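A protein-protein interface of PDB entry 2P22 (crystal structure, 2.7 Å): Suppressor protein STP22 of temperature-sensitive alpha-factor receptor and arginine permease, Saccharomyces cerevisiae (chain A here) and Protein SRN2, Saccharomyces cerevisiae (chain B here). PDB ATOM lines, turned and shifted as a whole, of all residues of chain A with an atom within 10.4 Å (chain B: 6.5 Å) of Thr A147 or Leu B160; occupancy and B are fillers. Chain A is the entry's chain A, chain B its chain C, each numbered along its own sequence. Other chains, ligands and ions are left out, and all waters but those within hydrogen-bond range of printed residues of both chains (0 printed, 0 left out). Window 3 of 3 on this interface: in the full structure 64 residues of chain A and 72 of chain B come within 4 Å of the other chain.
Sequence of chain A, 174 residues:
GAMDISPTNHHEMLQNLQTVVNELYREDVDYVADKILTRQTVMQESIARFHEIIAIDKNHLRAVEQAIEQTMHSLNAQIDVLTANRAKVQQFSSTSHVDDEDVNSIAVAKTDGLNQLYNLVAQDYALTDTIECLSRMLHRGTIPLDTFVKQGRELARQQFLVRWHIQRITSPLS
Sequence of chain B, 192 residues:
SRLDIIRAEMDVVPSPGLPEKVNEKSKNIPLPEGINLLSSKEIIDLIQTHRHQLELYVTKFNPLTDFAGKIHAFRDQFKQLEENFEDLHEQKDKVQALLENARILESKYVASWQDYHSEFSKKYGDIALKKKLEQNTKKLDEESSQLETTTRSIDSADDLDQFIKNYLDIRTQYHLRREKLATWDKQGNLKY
CD1 of Ile B154 touches CE of Met A137, at 3.5 Å. CE2 of Phe B163 touches SD of Met A137 (3.3 Å). CG2 of Thr A142 touches N of Ile B154 (3.8 Å). Ile A143 touches Leu B160. Thr A147 touches Leu B160. Leu B160 touches Gln A151 (CD2 to CG, 3.8 Å). Asp B161 touches Gln A151. Ile B164 touches Gln A151.
Hydrophobic or aromatic side chains of chain B that line the printed part of chain A: Ile B154, Leu B160, Phe B163 and Ile B164. Among the printed residues, no Asp or Glu carboxylate lies within 4 Å of a Lys or Arg side-chain nitrogen of the other chain.
Printed residues of chain B within 4 Å of Met A137: Ile B154 and Phe B163. Printed residues of chain B within 4 Å of Thr A142: Ile B154 (3.8 Å). Of the printed residues of chain B, Ile A143 touches Leu B160 (3.999 Å). Of the printed residues of chain B, Thr A147 touches Leu B160 (3.3 Å). No residue of chain A comes within 4 Å of Ala B157. No residue of chain A comes within 4 Å of Asp B159. The nearest printed residue of chain A that does not touch Leu B160 is Met A137 (4.3 Å).
O of Met A137 sits at hydrogen-bond distance from N of Thr A142 (2.8 Å). N of Ile A143 lies within hydrogen-bond range of O of Met A137 (3.3 Å).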
ATOM      1  N   THR A 130      18.837   1.730 -15.352  1.00  0.00           N
ATOM      2  CA  THR A 130      18.867   0.993 -16.583  1.00  0.00           C
ATOM      3  C   THR A 130      17.464   0.638 -17.001  1.00  0.00           C
ATOM      4  O   THR A 130      17.122   0.798 -18.162  1.00  0.00           O
ATOM      5  CB  THR A 130      19.709  -0.280 -16.451  1.00  0.00           C
ATOM      6  OG1 THR A 130      20.962   0.036 -15.828  1.00  0.00           O
ATOM      7  CG2 THR A 130      19.986  -0.859 -17.824  1.00  0.00           C
ATOM      8  N   ILE A 131      16.638   0.169 -16.068  1.00  0.00           N
ATOM      9  CA  ILE A 131      15.265  -0.180 -16.435  1.00  0.00           C
ATOM     10  C   ILE A 131      14.550   1.109 -16.842  1.00  0.00           C
ATOM     11  O   ILE A 131      13.802   1.126 -17.815  1.00  0.00           O
ATOM     12  CB  ILE A 131      14.503  -0.904 -15.274  1.00  0.00           C
ATOM     13  CG1 ILE A 131      15.320  -2.119 -14.790  1.00  0.00           C
ATOM     14  CG2 ILE A 131      13.142  -1.437 -15.782  1.00  0.00           C
ATOM     15  CD1 ILE A 131      14.712  -2.887 -13.599  1.00  0.00           C
ATOM     16  N   CYS A 133      15.793   3.875 -18.227  1.00  0.00           N
ATOM     17  CA  CYS A 133      16.293   4.185 -19.569  1.00  0.00           C
ATOM     18  C   CYS A 133      15.621   3.342 -20.644  1.00  0.00           C
ATOM     19  O   CYS A 133      15.064   3.876 -21.586  1.00  0.00           O
ATOM     20  CB  CYS A 133      17.800   3.952 -19.641  1.00  0.00           C
ATOM     21  SG  CYS A 133      18.462   4.029 -21.299  1.00  0.00           S
ATOM     22  N   LEU A 134      15.683   2.025 -20.513  1.00  0.00           N
ATOM     23  CA  LEU A 134      15.050   1.163 -21.486  1.00  0.00           C
ATOM     24  C   LEU A 134      13.588   1.525 -21.647  1.00  0.00           C
ATOM     25  O   LEU A 134      12.993   1.218 -22.666  1.00  0.00           O
ATOM     26  CB  LEU A 134      15.125  -0.297 -21.052  1.00  0.00           C
ATOM     27  CG  LEU A 134      16.283  -1.187 -21.497  1.00  0.00           C
ATOM     28  CD1 LEU A 134      17.551  -0.781 -20.781  1.00  0.00           C
ATOM     29  CD2 LEU A 134      15.954  -2.630 -21.194  1.00  0.00           C
ATOM     30  N   SER A 135      12.996   2.139 -20.628  1.00  0.00           N
ATOM     31  CA  SER A 135      11.578   2.517 -20.676  1.00  0.00           C
ATOM     32  C   SER A 135      11.460   3.617 -21.727  1.00  0.00           C
ATOM     33  O   SER A 135      10.574   3.626 -22.586  1.00  0.00           O
ATOM     34  CB  SER A 135      11.137   3.045 -19.300  1.00  0.00           C
ATOM     35  OG  SER A 135       9.761   3.382 -19.267  1.00  0.00           O
ATOM     36  N   MET A 137      13.693   4.222 -24.058  1.00  0.00           N
ATOM     37  CA  MET A 137      14.027   3.650 -25.359  1.00  0.00           C
ATOM     38  C   MET A 137      12.791   3.046 -26.022  1.00  0.00           C
ATOM     39  O   MET A 137      12.688   3.007 -27.244  1.00  0.00           O
ATOM     40  CB  MET A 137      15.080   2.554 -25.211  1.00  0.00           C
ATOM     41  CG  MET A 137      16.409   3.021 -24.676  1.00  0.00           C
ATOM     42  SD  MET A 137      17.472   1.617 -24.260  1.00  0.00           S
ATOM     43  CE  MET A 137      18.033   1.112 -25.898  1.00  0.00           C
ATOM     44  N   LEU A 138      11.863   2.559 -25.210  1.00  0.00           N
ATOM     45  CA  LEU A 138      10.652   1.969 -25.739  1.00  0.00           C
ATOM     46  C   LEU A 138       9.743   3.096 -26.203  1.00  0.00           C
ATOM     47  O   LEU A 138       9.099   3.000 -27.245  1.00  0.00           O
ATOM     48  CB  LEU A 138       9.950   1.140 -24.665  1.00  0.00           C
ATOM     49  CG  LEU A 138       8.572   0.565 -25.013  1.00  0.00           C
ATOM     50  CD1 LEU A 138       8.670  -0.342 -26.229  1.00  0.00           C
ATOM     51  CD2 LEU A 138       8.022  -0.209 -23.830  1.00  0.00           C
ATOM     52  N   GLY A 141      10.813   4.530 -29.332  1.00  0.00           N
ATOM     53  CA  GLY A 141      10.640   3.583 -30.422  1.00  0.00           C
ATOM     54  C   GLY A 141      11.927   2.846 -30.769  1.00  0.00           C
ATOM     55  O   GLY A 141      11.954   2.073 -31.721  1.00  0.00           O
ATOM     56  N   THR A 142      12.988   3.085 -30.000  1.00  0.00           N
ATOM     57  CA  THR A 142      14.284   2.442 -30.210  1.00  0.00           C
ATOM     58  C   THR A 142      14.241   0.919 -30.008  1.00  0.00           C
ATOM     59  O   THR A 142      15.140   0.206 -30.462  1.00  0.00           O
ATOM     60  CB  THR A 142      15.356   3.016 -29.247  1.00  0.00           C
ATOM     61  OG1 THR A 142      15.429   4.442 -29.390  1.00  0.00           O
ATOM     62  CG2 THR A 142      16.725   2.406 -29.544  1.00  0.00           C
ATOM     63  N   ILE A 143      13.216   0.430 -29.308  1.00  0.00           N
ATOM     64  CA  ILE A 143      13.036  -1.007 -29.053  1.00  0.00           C
ATOM     65  C   ILE A 143      11.550  -1.332 -28.884  1.00  0.00           C
ATOM     66  O   ILE A 143      10.807  -0.561 -28.284  1.00  0.00           O
ATOM     67  CB  ILE A 143      13.782  -1.476 -27.761  1.00  0.00           C
ATOM     68  CG1 ILE A 143      13.312  -0.647 -26.559  1.00  0.00           C
ATOM     69  CG2 ILE A 143      15.303  -1.359 -27.944  1.00  0.00           C
ATOM     70  CD1 ILE A 143      13.827  -1.145 -25.216  1.00  0.00           C
ATOM     71  N   PRO A 144      11.094  -2.475 -29.426  1.00  0.00           N
ATOM     72  CA  PRO A 144       9.688  -2.873 -29.314  1.00  0.00           C
ATOM     73  C   PRO A 144       9.363  -3.369 -27.920  1.00  0.00           C
ATOM     74  O   PRO A 144      10.254  -3.773 -27.174  1.00  0.00           O
ATOM     75  CB  PRO A 144       9.551  -3.982 -30.355  1.00  0.00           C
ATOM     76  CG  PRO A 144      10.876  -4.626 -30.315  1.00  0.00           C
ATOM     77  CD  PRO A 144      11.832  -3.432 -30.266  1.00  0.00           C
ATOM     78  N   LEU A 145       8.077  -3.338 -27.586  1.00  0.00           N
ATOM     79  CA  LEU A 145       7.592  -3.773 -26.284  1.00  0.00           C
ATOM     80  C   LEU A 145       8.090  -5.173 -25.958  1.00  0.00           C
ATOM     81  O   LEU A 145       8.357  -5.505 -24.800  1.00  0.00           O
ATOM     82  CB  LEU A 145       6.065  -3.776 -26.274  1.00  0.00           C
ATOM     83  CG  LEU A 145       5.438  -4.197 -24.947  1.00  0.00           C
ATOM     84  CD1 LEU A 145       5.448  -3.027 -23.979  1.00  0.00           C
ATOM     85  CD2 LEU A 145       4.042  -4.675 -25.186  1.00  0.00           C
ATOM     86  N   ASP A 146       8.201  -5.991 -26.997  1.00  0.00           N
ATOM     87  CA  ASP A 146       8.656  -7.364 -26.864  1.00  0.00           C
ATOM     88  C   ASP A 146      10.036  -7.411 -26.212  1.00  0.00           C
ATOM     89  O   ASP A 146      10.273  -8.176 -25.275  1.00  0.00           O
ATOM     90  CB  ASP A 146       8.698  -8.011 -28.245  1.00  0.00           C
ATOM     91  CG  ASP A 146       8.687  -9.514 -28.180  1.00  0.00           C
ATOM     92  OD1 ASP A 146       9.615 -10.085 -27.571  1.00  0.00           O
ATOM     93  OD2 ASP A 146       7.747 -10.122 -28.735  1.00  0.00           O
ATOM     94  N   THR A 147      10.945  -6.583 -26.710  1.00  0.00           N
ATOM     95  CA  THR A 147      12.286  -6.540 -26.169  1.00  0.00           C
ATOM     96  C   THR A 147      12.302  -5.995 -24.751  1.00  0.00           C
ATOM     97  O   THR A 147      12.901  -6.591 -23.858  1.00  0.00           O
ATOM     98  CB  THR A 147      13.205  -5.673 -27.035  1.00  0.00           C
ATOM     99  OG1 THR A 147      13.310  -6.252 -28.336  1.00  0.00           O
ATOM    100  CG2 THR A 147      14.591  -5.583 -26.424  1.00  0.00           C
ATOM    101  N   PHE A 148      11.639  -4.862 -24.543  1.00  0.00           N
ATOM    102  CA  PHE A 148      11.593  -4.232 -23.223  1.00  0.00           C
ATOM    103  C   PHE A 148      11.235  -5.182 -22.086  1.00  0.00           C
ATOM    104  O   PHE A 148      11.835  -5.135 -21.011  1.00  0.00           O
ATOM    105  CB  PHE A 148      10.586  -3.083 -23.202  1.00  0.00           C
ATOM    106  CG  PHE A 148      10.406  -2.484 -21.837  1.00  0.00           C
ATOM    107  CD1 PHE A 148      11.327  -1.572 -21.338  1.00  0.00           C
ATOM    108  CD2 PHE A 148       9.351  -2.879 -21.024  1.00  0.00           C
ATOM    109  CE1 PHE A 148      11.203  -1.060 -20.053  1.00  0.00           C
ATOM    110  CE2 PHE A 148       9.220  -2.373 -19.736  1.00  0.00           C
ATOM    111  CZ  PHE A 148      10.149  -1.462 -19.253  1.00  0.00           C
ATOM    112  N   VAL A 149      10.237  -6.021 -22.326  1.00  0.00           N
ATOM    113  CA  VAL A 149       9.786  -6.962 -21.326  1.00  0.00           C
ATOM    114  C   VAL A 149      10.851  -7.986 -20.943  1.00  0.00           C
ATOM    115  O   VAL A 149      11.142  -8.177 -19.760  1.00  0.00           O
ATOM    116  CB  VAL A 149       8.539  -7.690 -21.809  1.00  0.00           C
ATOM    117  CG1 VAL A 149       8.074  -8.674 -20.753  1.00  0.00           C
ATOM    118  CG2 VAL A 149       7.449  -6.672 -22.125  1.00  0.00           C
ATOM    119  N   LYS A 150      11.434  -8.642 -21.943  1.00  0.00           N
ATOM    120  CA  LYS A 150      12.463  -9.645 -21.687  1.00  0.00           C
ATOM    121  C   LYS A 150      13.605  -9.075 -20.871  1.00  0.00           C
ATOM    122  O   LYS A 150      13.850  -9.516 -19.748  1.00  0.00           O
ATOM    123  CB  LYS A 150      13.012 -10.217 -23.002  1.00  0.00           C
ATOM    124  CG  LYS A 150      14.304 -11.025 -22.838  1.00  0.00           C
ATOM    125  CD  LYS A 150      14.639 -11.883 -24.067  1.00  0.00           C
ATOM    126  CE  LYS A 150      13.646 -13.038 -24.269  1.00  0.00           C
ATOM    127  NZ  LYS A 150      13.695 -14.091 -23.204  1.00  0.00           N
ATOM    128  N   GLN A 151      14.299  -8.095 -21.438  1.00  0.00           N
ATOM    129  CA  GLN A 151      15.430  -7.472 -20.768  1.00  0.00           C
ATOM    130  C   GLN A 151      14.982  -6.829 -19.469  1.00  0.00           C
ATOM    131  O   GLN A 151      15.707  -6.850 -18.474  1.00  0.00           O
ATOM    132  CB  GLN A 151      16.071  -6.409 -21.668  1.00  0.00           C
ATOM    133  CG  GLN A 151      16.436  -6.891 -23.068  1.00  0.00           C
ATOM    134  CD  GLN A 151      17.426  -8.041 -23.062  1.00  0.00           C
ATOM    135  OE1 GLN A 151      18.585  -7.874 -22.671  1.00  0.00           O
ATOM    136  NE2 GLN A 151      16.971  -9.223 -23.492  1.00  0.00           N
ATOM    137  N   GLY A 152      13.784  -6.253 -19.493  1.00  0.00           N
ATOM    138  CA  GLY A 152      13.236  -5.599 -18.318  1.00  0.00           C
ATOM    139  C   GLY A 152      13.096  -6.580 -17.178  1.00  0.00           C
ATOM    140  O   GLY A 152      13.584  -6.335 -16.084  1.00  0.00           O
ATOM    141  N   ARG A 153      12.418  -7.690 -17.433  1.00  0.00           N
ATOM    142  CA  ARG A 153      12.252  -8.707 -16.411  1.00  0.00           C
ATOM    143  C   ARG A 153      13.605  -9.195 -15.895  1.00  0.00           C
ATOM    144  O   ARG A 153      13.719  -9.557 -14.730  1.00  0.00           O
ATOM    145  CB  ARG A 153      11.481  -9.894 -16.965  1.00  0.00           C
ATOM    146  CG  ARG A 153       9.986  -9.741 -16.913  1.00  0.00           C
ATOM    147  CD  ARG A 153       9.387 -10.868 -16.097  1.00  0.00           C
ATOM    148  NE  ARG A 153       9.548 -12.168 -16.740  1.00  0.00           N
ATOM    149  CZ  ARG A 153       9.158 -13.316 -16.196  1.00  0.00           C
ATOM    150  NH1 ARG A 153       8.593 -13.315 -15.001  1.00  0.00           N
ATOM    151  NH2 ARG A 153       9.325 -14.461 -16.849  1.00  0.00           N
ATOM    152  N   GLU A 154      14.626  -9.197 -16.756  1.00  0.00           N
ATOM    153  CA  GLU A 154      15.958  -9.660 -16.370  1.00  0.00           C
ATOM    154  C   GLU A 154      16.670  -8.715 -15.420  1.00  0.00           C
ATOM    155  O   GLU A 154      17.227  -9.141 -14.410  1.00  0.00           O
ATOM    156  CB  GLU A 154      16.835  -9.909 -17.611  1.00  0.00           C
ATOM    157  CG  GLU A 154      18.311 -10.369 -17.348  1.00  0.00           C
ATOM    158  CD  GLU A 154      18.466 -11.611 -16.434  1.00  0.00           C
ATOM    159  OE1 GLU A 154      17.487 -12.377 -16.235  1.00  0.00           O
ATOM    160  OE2 GLU A 154      19.598 -11.821 -15.922  1.00  0.00           O
ATOM    161  N   LEU A 155      16.674  -7.431 -15.736  1.00  0.00           N
ATOM    162  CA  LEU A 155      17.336  -6.470 -14.865  1.00  0.00           C
ATOM    163  C   LEU A 155      16.577  -6.323 -13.548  1.00  0.00           C
ATOM    164  O   LEU A 155      17.172  -6.065 -12.511  1.00  0.00           O
ATOM    165  CB  LEU A 155      17.419  -5.122 -15.563  1.00  0.00           C
ATOM    166  CG  LEU A 155      18.339  -5.103 -16.771  1.00  0.00           C
ATOM    167  CD1 LEU A 155      18.145  -3.810 -17.537  1.00  0.00           C
ATOM    168  CD2 LEU A 155      19.773  -5.252 -16.300  1.00  0.00           C
ATOM    169  N   ILE B 154      18.720   0.469 -32.114  1.00  0.00           N
ATOM    170  CA  ILE B 154      19.491  -0.751 -31.909  1.00  0.00           C
ATOM    171  C   ILE B 154      18.772  -1.933 -32.546  1.00  0.00           C
ATOM    172  O   ILE B 154      17.999  -2.633 -31.888  1.00  0.00           O
ATOM    173  CB  ILE B 154      19.669  -1.054 -30.408  1.00  0.00           C
ATOM    174  CG1 ILE B 154      20.259   0.162 -29.696  1.00  0.00           C
ATOM    175  CG2 ILE B 154      20.576  -2.263 -30.224  1.00  0.00           C
ATOM    176  CD1 ILE B 154      20.400  -0.023 -28.203  1.00  0.00           C
ATOM    177  N   SER B 156      20.459  -4.415 -33.960  1.00  0.00           N
ATOM    178  CA  SER B 156      21.308  -5.566 -33.671  1.00  0.00           C
ATOM    179  C   SER B 156      21.079  -6.057 -32.244  1.00  0.00           C
ATOM    180  O   SER B 156      21.432  -5.378 -31.281  1.00  0.00           O
ATOM    181  CB  SER B 156      22.775  -5.186 -33.860  1.00  0.00           C
ATOM    182  OG  SER B 156      22.975  -4.603 -35.134  1.00  0.00           O
ATOM    183  N   ALA B 157      20.485  -7.238 -32.117  1.00  0.00           N
ATOM    184  CA  ALA B 157      20.196  -7.812 -30.809  1.00  0.00           C
ATOM    185  C   ALA B 157      21.428  -7.809 -29.913  1.00  0.00           C
ATOM    186  O   ALA B 157      21.350  -7.436 -28.742  1.00  0.00           O
ATOM    187  CB  ALA B 157      19.670  -9.229 -30.970  1.00  0.00           C
ATOM    188  N   ASP B 158      22.560  -8.223 -30.471  1.00  0.00           N
ATOM    189  CA  ASP B 158      23.819  -8.278 -29.733  1.00  0.00           C
ATOM    190  C   ASP B 158      24.180  -6.901 -29.173  1.00  0.00           C
ATOM    191  O   ASP B 158      24.560  -6.776 -28.008  1.00  0.00           O
ATOM    192  CB  ASP B 158      24.941  -8.781 -30.655  1.00  0.00           C
ATOM    193  CG  ASP B 158      26.251  -9.034 -29.913  1.00  0.00           C
ATOM    194  OD1 ASP B 158      27.266  -9.321 -30.583  1.00  0.00           O
ATOM    195  OD2 ASP B 158      26.265  -8.954 -28.667  1.00  0.00           O
ATOM    196  N   ASP B 159      24.059  -5.875 -30.009  1.00  0.00           N
ATOM    197  CA  ASP B 159      24.370  -4.507 -29.599  1.00  0.00           C
ATOM    198  C   ASP B 159      23.625  -4.119 -28.329  1.00  0.00           C
ATOM    199  O   ASP B 159      24.182  -3.460 -27.454  1.00  0.00           O
ATOM    200  CB  ASP B 159      24.016  -3.522 -30.718  1.00  0.00           C
ATOM    201  CG  ASP B 159      25.036  -3.518 -31.836  1.00  0.00           C
ATOM    202  OD1 ASP B 159      25.330  -4.604 -32.380  1.00  0.00           O
ATOM    203  OD2 ASP B 159      25.542  -2.426 -32.174  1.00  0.00           O
ATOM    204  N   LEU B 160      22.364  -4.529 -28.237  1.00  0.00           N
ATOM    205  CA  LEU B 160      21.549  -4.221 -27.072  1.00  0.00           C
ATOM    206  C   LEU B 160      22.321  -4.590 -25.814  1.00  0.00           C
ATOM    207  O   LEU B 160      22.640  -3.728 -24.999  1.00  0.00           O
ATOM    208  CB  LEU B 160      20.239  -5.003 -27.118  1.00  0.00           C
ATOM    209  CG  LEU B 160      19.112  -4.444 -26.244  1.00  0.00           C
ATOM    210  CD1 LEU B 160      18.717  -3.078 -26.768  1.00  0.00           C
ATOM    211  CD2 LEU B 160      17.895  -5.377 -26.263  1.00  0.00           C
ATOM    212  N   ASP B 161      22.632  -5.871 -25.666  1.00  0.00           N
ATOM    213  CA  ASP B 161      23.373  -6.327 -24.502  1.00  0.00           C
ATOM    214  C   ASP B 161      24.588  -5.462 -24.227  1.00  0.00           C
ATOM    215  O   ASP B 161      24.844  -5.086 -23.083  1.00  0.00           O
ATOM    216  CB  ASP B 161      23.825  -7.775 -24.675  1.00  0.00           C
ATOM    217  CG  ASP B 161      22.702  -8.758 -24.462  1.00  0.00           C
ATOM    218  OD1 ASP B 161      22.097  -8.745 -23.368  1.00  0.00           O
ATOM    219  OD2 ASP B 161      22.425  -9.546 -25.387  1.00  0.00           O
ATOM    220  N   GLN B 162      25.339  -5.147 -25.275  1.00  0.00           N
ATOM    221  CA  GLN B 162      26.535  -4.329 -25.112  1.00  0.00           C
ATOM    222  C   GLN B 162      26.148  -2.966 -24.574  1.00  0.00           C
ATOM    223  O   GLN B 162      26.829  -2.410 -23.723  1.00  0.00           O
ATOM    224  CB  GLN B 162      27.270  -4.185 -26.446  1.00  0.00           C
ATOM    225  CG  GLN B 162      27.586  -5.525 -27.096  1.00  0.00           C
ATOM    226  CD  GLN B 162      28.382  -6.453 -26.181  1.00  0.00           C
ATOM    227  OE1 GLN B 162      29.601  -6.310 -26.031  1.00  0.00           O
ATOM    228  NE2 GLN B 162      27.690  -7.402 -25.552  1.00  0.00           N
ATOM    229  N   PHE B 163      25.037  -2.442 -25.069  1.00  0.00           N
ATOM    230  CA  PHE B 163      24.549  -1.147 -24.629  1.00  0.00           C
ATOM    231  C   PHE B 163      24.163  -1.192 -23.153  1.00  0.00           C
ATOM    232  O   PHE B 163      24.620  -0.381 -22.345  1.00  0.00           O
ATOM    233  CB  PHE B 163      23.336  -0.757 -25.451  1.00  0.00           C
ATOM    234  CG  PHE B 163      22.614   0.419 -24.908  1.00  0.00           C
ATOM    235  CD1 PHE B 163      23.198   1.681 -24.948  1.00  0.00           C
ATOM    236  CD2 PHE B 163      21.367   0.266 -24.314  1.00  0.00           C
ATOM    237  CE1 PHE B 163      22.550   2.772 -24.404  1.00  0.00           C
ATOM    238  CE2 PHE B 163      20.711   1.349 -23.766  1.00  0.00           C
ATOM    239  CZ  PHE B 163      21.301   2.608 -23.809  1.00  0.00           C
ATOM    240  N   ILE B 164      23.295  -2.138 -22.820  1.00  0.00           N
ATOM    241  CA  ILE B 164      22.847  -2.331 -21.455  1.00  0.00           C
ATOM    242  C   ILE B 164      24.024  -2.506 -20.487  1.00  0.00           C
ATOM    243  O   ILE B 164      24.064  -1.862 -19.438  1.00  0.00           O
ATOM    244  CB  ILE B 164      21.957  -3.567 -21.366  1.00  0.00           C
ATOM    245  CG1 ILE B 164      20.702  -3.341 -22.211  1.00  0.00           C
ATOM    246  CG2 ILE B 164      21.656  -3.893 -19.909  1.00  0.00           C
ATOM    247  CD1 ILE B 164      19.760  -4.515 -22.232  1.00  0.00           C
ATOM    248  N   LYS B 165      24.977  -3.373 -20.833  1.00  0.00           N
ATOM    249  CA  LYS B 165      26.139  -3.614 -19.968  1.00  0.00           C
ATOM    250  C   LYS B 165      26.925  -2.340 -19.710  1.00  0.00           C
ATOM    251  O   LYS B 165      27.324  -2.060 -18.576  1.00  0.00           O
ATOM    252  CB  LYS B 165      27.089  -4.661 -20.579  1.00  0.00           C
ATOM    253  CG  LYS B 165      26.525  -6.084 -20.665  1.00  0.00           C
ATOM    254  CD  LYS B 165      27.590  -7.113 -21.069  1.00  0.00           C
ATOM    255  CE  LYS B 165      26.997  -8.519 -21.270  1.00  0.00           C
ATOM    256  NZ  LYS B 165      26.097  -8.638 -22.466  1.00  0.00           N
